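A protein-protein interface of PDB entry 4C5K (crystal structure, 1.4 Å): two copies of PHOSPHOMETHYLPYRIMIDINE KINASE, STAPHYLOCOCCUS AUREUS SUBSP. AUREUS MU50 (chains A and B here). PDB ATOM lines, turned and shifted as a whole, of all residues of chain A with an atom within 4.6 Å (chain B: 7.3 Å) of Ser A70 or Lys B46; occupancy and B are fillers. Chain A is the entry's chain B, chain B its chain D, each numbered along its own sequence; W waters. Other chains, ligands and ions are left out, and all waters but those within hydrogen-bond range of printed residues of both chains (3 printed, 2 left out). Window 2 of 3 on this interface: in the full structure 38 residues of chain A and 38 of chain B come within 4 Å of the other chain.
Water W1 bridges OD2 of Asp B45 (2.7 Å) and OE2 of Glu A66 (2.9 Å). Water W3 lies within hydrogen-bond range of the side-chain hydroxyl of Ser A70 (2.7 Å) and the side-chain amide nitrogen of Asn B252 (2.9 Å). Water W2 lies within hydrogen-bond range of the backbone carbonyl oxygen (O) of Met B44 (3.0 Å) and the side-chain hydroxyl (OG1) of Thr A67 (3.3 Å).
Of the 7 printed residues of chain A, 4 touch a printed residue of chain B. Hydrophobic or aromatic side chains of chain A that line the printed part of chain B: Ile A71. Among the printed residues, no Asp or Glu carboxylate lies within 4 Å of a Lys or Arg side-chain nitrogen of the other chain.
OD1 of Asp B45 lies within hydrogen-bond range of N of Thr B48, at 3.1 Å. The backbone carbonyl oxygen (O) of Ser B50 sits at hydrogen-bond distance from the backbone NH (N) of Asp B45 (2.9 Å). N of Asp B47 lies within hydrogen-bond range of OD1 of Asp B45 (2.8 Å). NZ of Lys B46 lies within salt-bridge range of OD2 of Asp B47, at 3.2 Å.
No position is printed for both chains.
OE2 of Glu A66 is in hydrogen-bond range of N of Lys B46. O of Met B44 lies within hydrogen-bond range of OG1 of Thr A67 (2.8 Å).
Of the printed residues of chain B, Thr A67 touches Met B44 (2.8 Å) and Trp B49 (3.9 Å). Ser A70 touches just these residues of chain B: Lys B46 and Trp B49. Gly A72 touches none of the printed residues of chain B. Of the printed residues of chain A, Met B251 touches Ile A71. Phe B254 touches none of the printed residues of chain A. The nearest printed residue of chain A that does not touch Lys B46 is Thr A67 (5.8 Å). The nearest printed residue of chain A that does not touch Met B44 is Glu A66 (4.1 Å).
CA of Asp B45 touches OE2 of Glu A66 (3.6 Å). Thr A67 touches Trp B49. Ser A70 touches Lys B46 (OG to O, 3.7 Å). CZ3 of Trp B49 touches OG of Ser A70 (3.7 Å). Trp B49 touches Ile A71 (CH2 to CG1, 3.7 Å). CD1 of Ile A71 touches SD of Met B251, at 3.7 Å.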
ATOM      1  N   GLU A  66     -20.779 -19.281  16.621  1.00  0.00           N
ATOM      2  CA  GLU A  66     -21.923 -19.993  17.169  1.00  0.00           C
ATOM      3  C   GLU A  66     -21.986 -19.792  18.697  1.00  0.00           C
ATOM      4  O   GLU A  66     -23.034 -19.516  19.275  1.00  0.00           O
ATOM      5  CB  GLU A  66     -21.853 -21.504  16.853  1.00  0.00           C
ATOM      6  CG  GLU A  66     -22.794 -22.372  17.706  1.00  0.00           C
ATOM      7  CD  GLU A  66     -22.842 -23.840  17.293  1.00  0.00           C
ATOM      8  OE1 GLU A  66     -22.792 -24.150  16.066  1.00  0.00           O
ATOM      9  OE2 GLU A  66     -22.954 -24.685  18.213  1.00  0.00           O
ATOM     10  N   THR A  67     -20.853 -19.939  19.336  1.00  0.00           N
ATOM     11  CA  THR A  67     -20.798 -19.737  20.798  1.00  0.00           C
ATOM     12  C   THR A  67     -21.198 -18.313  21.185  1.00  0.00           C
ATOM     13  O   THR A  67     -22.049 -18.089  22.065  1.00  0.00           O
ATOM     14  CB  THR A  67     -19.429 -20.100  21.341  1.00  0.00           C
ATOM     15  OG1 THR A  67     -19.140 -21.462  21.017  1.00  0.00           O
ATOM     16  CG2 THR A  67     -19.321 -19.868  22.825  1.00  0.00           C
ATOM     17  N   ALA A  68     -20.592 -17.342  20.514  1.00  0.00           N
ATOM     18  CA  ALA A  68     -20.886 -15.936  20.819  1.00  0.00           C
ATOM     19  C   ALA A  68     -22.336 -15.539  20.561  1.00  0.00           C
ATOM     20  O   ALA A  68     -22.941 -14.837  21.372  1.00  0.00           O
ATOM     21  CB  ALA A  68     -19.967 -15.039  20.016  1.00  0.00           C
ATOM     22  N   LEU A  69     -22.905 -16.029  19.447  1.00  0.00           N
ATOM     23  CA  LEU A  69     -24.280 -15.748  19.137  1.00  0.00           C
ATOM     24  C   LEU A  69     -25.202 -16.346  20.220  1.00  0.00           C
ATOM     25  O   LEU A  69     -26.220 -15.740  20.601  1.00  0.00           O
ATOM     26  CB  LEU A  69     -24.657 -16.250  17.724  1.00  0.00           C
ATOM     27  CG  LEU A  69     -26.136 -16.112  17.345  1.00  0.00           C
ATOM     28  CD1 LEU A  69     -26.619 -14.662  17.316  1.00  0.00           C
ATOM     29  CD2 LEU A  69     -26.429 -16.759  15.990  1.00  0.00           C
ATOM     30  N   SER A  70     -24.866 -17.555  20.674  1.00  0.00           N
ATOM     31  CA  SER A  70     -25.663 -18.231  21.702  1.00  0.00           C
ATOM     32  C   SER A  70     -25.693 -17.453  23.014  1.00  0.00           C
ATOM     33  O   SER A  70     -26.743 -17.295  23.615  1.00  0.00           O
ATOM     34  CB  SER A  70     -25.123 -19.617  21.927  1.00  0.00           C
ATOM     35  OG  SER A  70     -25.861 -20.326  22.917  1.00  0.00           O
ATOM     36  N   ILE A  71     -24.537 -16.913  23.386  1.00  0.00           N
ATOM     37  CA  ILE A  71     -24.390 -16.052  24.569  1.00  0.00           C
ATOM     38  C   ILE A  71     -25.272 -14.797  24.462  1.00  0.00           C
ATOM     39  O   ILE A  71     -25.906 -14.381  25.399  1.00  0.00           O
ATOM     40  CB  ILE A  71     -22.907 -15.752  24.841  1.00  0.00           C
ATOM     41  CG1 ILE A  71     -22.210 -17.042  25.284  1.00  0.00           C
ATOM     42  CG2 ILE A  71     -22.748 -14.670  25.894  1.00  0.00           C
ATOM     43  CD1 ILE A  71     -20.737 -16.963  25.274  1.00  0.00           C
ATOM     44  N   GLY A  72     -25.261 -14.200  23.274  1.00  0.00           N
ATOM     45  CA  GLY A  72     -26.140 -13.098  22.935  1.00  0.00           C
ATOM     46  C   GLY A  72     -25.528 -11.756  23.220  1.00  0.00           C
ATOM     47  O   GLY A  72     -25.779 -11.165  24.268  1.00  0.00           O
ATOM     48  N   MET B  44     -17.959 -23.822  22.261  1.00  0.00           N
ATOM     49  CA  MET B  44     -19.009 -24.522  22.980  1.00  0.00           C
ATOM     50  C   MET B  44     -20.237 -24.674  22.108  1.00  0.00           C
ATOM     51  O   MET B  44     -20.690 -23.728  21.453  1.00  0.00           O
ATOM     52  CB  MET B  44     -19.382 -23.838  24.295  1.00  0.00           C
ATOM     53  CG  MET B  44     -18.298 -23.722  25.329  1.00  0.00           C
ATOM     54  SD  MET B  44     -17.139 -22.363  25.017  1.00  0.00           S
ATOM     55  CE  MET B  44     -15.970 -22.684  26.311  1.00  0.00           C
ATOM     56  N   ASP B  45     -20.808 -25.873  22.104  1.00  0.00           N
ATOM     57  CA  ASP B  45     -22.035 -26.132  21.343  1.00  0.00           C
ATOM     58  C   ASP B  45     -23.210 -25.340  21.870  1.00  0.00           C
ATOM     59  O   ASP B  45     -23.454 -25.284  23.090  1.00  0.00           O
ATOM     60  CB  ASP B  45     -22.329 -27.626  21.387  1.00  0.00           C
ATOM     61  CG  ASP B  45     -23.569 -28.000  20.587  1.00  0.00           C
ATOM     62  OD1 ASP B  45     -24.659 -27.967  21.098  1.00  0.00           O
ATOM     63  OD2 ASP B  45     -23.385 -28.283  19.401  1.00  0.00           O
ATOM     64  N   LYS B  46     -23.934 -24.664  20.963  1.00  0.00           N
ATOM     65  CA  LYS B  46     -25.053 -23.829  21.392  1.00  0.00           C
ATOM     66  C   LYS B  46     -26.171 -24.549  22.199  1.00  0.00           C
ATOM     67  O   LYS B  46     -26.908 -23.899  22.956  1.00  0.00           O
ATOM     68  CB  LYS B  46     -25.649 -23.107  20.185  1.00  0.00           C
ATOM     69  CG  LYS B  46     -26.371 -23.993  19.225  1.00  0.00           C
ATOM     70  CD  LYS B  46     -26.857 -23.213  18.012  1.00  0.00           C
ATOM     71  CE  LYS B  46     -27.394 -24.164  16.982  1.00  0.00           C
ATOM     72  NZ  LYS B  46     -28.703 -24.670  17.441  1.00  0.00           N
ATOM     73  N   ASP B  47     -26.330 -25.850  21.993  1.00  0.00           N
ATOM     74  CA  ASP B  47     -27.403 -26.611  22.618  1.00  0.00           C
ATOM     75  C   ASP B  47     -26.995 -27.359  23.897  1.00  0.00           C
ATOM     76  O   ASP B  47     -27.839 -27.473  24.796  1.00  0.00           O
ATOM     77  CB  ASP B  47     -27.988 -27.598  21.616  1.00  0.00           C
ATOM     78  CG  ASP B  47     -28.636 -26.887  20.444  1.00  0.00           C
ATOM     79  OD1 ASP B  47     -29.440 -25.979  20.691  1.00  0.00           O
ATOM     80  OD2 ASP B  47     -28.295 -27.239  19.311  1.00  0.00           O
ATOM     81  N   THR B  48     -25.773 -27.880  23.953  1.00  0.00           N
ATOM     82  CA  THR B  48     -25.295 -28.705  25.082  1.00  0.00           C
ATOM     83  C   THR B  48     -24.162 -28.066  25.891  1.00  0.00           C
ATOM     84  O   THR B  48     -23.830 -28.536  26.989  1.00  0.00           O
ATOM     85  CB  THR B  48     -24.775 -30.046  24.575  1.00  0.00           C
ATOM     86  OG1 THR B  48     -23.633 -29.847  23.714  1.00  0.00           O
ATOM     87  CG2 THR B  48     -25.876 -30.778  23.861  1.00  0.00           C
ATOM     88  N   TRP B  49     -23.522 -27.063  25.293  1.00  0.00           N
ATOM     89  CA  TRP B  49     -22.333 -26.410  25.865  1.00  0.00           C
ATOM     90  C   TRP B  49     -21.134 -27.320  25.882  1.00  0.00           C
ATOM     91  O   TRP B  49     -20.099 -26.992  26.491  1.00  0.00           O
ATOM     92  CB  TRP B  49     -22.609 -25.806  27.258  1.00  0.00           C
ATOM     93  CG  TRP B  49     -21.926 -24.443  27.352  1.00  0.00           C
ATOM     94  CD1 TRP B  49     -20.893 -24.083  28.197  1.00  0.00           C
ATOM     95  CD2 TRP B  49     -22.163 -23.305  26.532  1.00  0.00           C
ATOM     96  NE1 TRP B  49     -20.510 -22.771  27.957  1.00  0.00           N
ATOM     97  CE2 TRP B  49     -21.267 -22.282  26.935  1.00  0.00           C
ATOM     98  CE3 TRP B  49     -23.047 -23.048  25.500  1.00  0.00           C
ATOM     99  CZ2 TRP B  49     -21.257 -21.013  26.348  1.00  0.00           C
ATOM    100  CZ3 TRP B  49     -23.028 -21.766  24.897  1.00  0.00           C
ATOM    101  CH2 TRP B  49     -22.154 -20.777  25.339  1.00  0.00           C
ATOM    102  N   SER B  50     -21.225 -28.445  25.163  1.00  0.00           N
ATOM    103  CA  SER B  50     -20.086 -29.362  25.032  1.00  0.00           C
ATOM    104  C   SER B  50     -18.898 -28.599  24.400  1.00  0.00           C
ATOM    105  O   SER B  50     -19.075 -27.840  23.428  1.00  0.00           O
ATOM    106  CB  SER B  50     -20.476 -30.568  24.179  1.00  0.00           C
ATOM    107  OG  SER B  50     -19.485 -31.536  24.308  1.00  0.00           O
ATOM    108  N   MET B 251     -24.893 -17.025  32.657  1.00  0.00           N
ATOM    109  CA  MET B 251     -24.787 -16.860  31.181  1.00  0.00           C
ATOM    110  C   MET B 251     -25.813 -17.676  30.400  1.00  0.00           C
ATOM    111  O   MET B 251     -26.399 -17.207  29.400  1.00  0.00           O
ATOM    112  CB  MET B 251     -23.353 -17.171  30.766  1.00  0.00           C
ATOM    113  CG  MET B 251     -23.109 -17.251  29.285  1.00  0.00           C
ATOM    114  SD  MET B 251     -21.356 -17.397  28.880  1.00  0.00           S
ATOM    115  CE  MET B 251     -20.822 -15.716  29.191  1.00  0.00           C
ATOM    116  N   ASN B 252     -26.047 -18.897  30.852  1.00  0.00           N
ATOM    117  CA  ASN B 252     -27.039 -19.761  30.271  1.00  0.00           C
ATOM    118  C   ASN B 252     -27.265 -20.884  31.284  1.00  0.00           C
ATOM    119  O   ASN B 252     -26.793 -20.764  32.418  1.00  0.00           O
ATOM    120  CB  ASN B 252     -26.615 -20.259  28.867  1.00  0.00           C
ATOM    121  CG  ASN B 252     -25.290 -20.978  28.888  1.00  0.00           C
ATOM    122  OD1 ASN B 252     -24.956 -21.651  29.851  1.00  0.00           O
ATOM    123  ND2 ASN B 252     -24.505 -20.829  27.799  1.00  0.00           N
ATOM    124  N   PHE B 254     -25.955 -23.620  31.520  1.00  0.00           N
ATOM    125  CA  PHE B 254     -24.741 -24.460  31.580  1.00  0.00           C
ATOM    126  C   PHE B 254     -23.507 -23.807  32.224  1.00  0.00           C
ATOM    127  O   PHE B 254     -22.559 -24.504  32.607  1.00  0.00           O
ATOM    128  CB  PHE B 254     -24.370 -24.986  30.164  1.00  0.00           C
ATOM    129  CG  PHE B 254     -25.549 -25.431  29.389  1.00  0.00           C
ATOM    130  CD1 PHE B 254     -26.268 -26.531  29.817  1.00  0.00           C
ATOM    131  CD2 PHE B 254     -25.957 -24.758  28.257  1.00  0.00           C
ATOM    132  CE1 PHE B 254     -27.411 -26.939  29.179  1.00  0.00           C
ATOM    133  CE2 PHE B 254     -27.086 -25.192  27.573  1.00  0.00           C
ATOM    134  CZ  PHE B 254     -27.809 -26.287  28.044  1.00  0.00           C
HETATM  135  O   HOH W   1     -21.530 -27.204  17.761  1.00  0.00           O
HETATM  136  O   HOH W   2     -19.611 -23.707  18.621  1.00  0.00           O
HETATM  137  O   HOH W   3     -26.070 -19.724  25.592  1.00  0.00           O
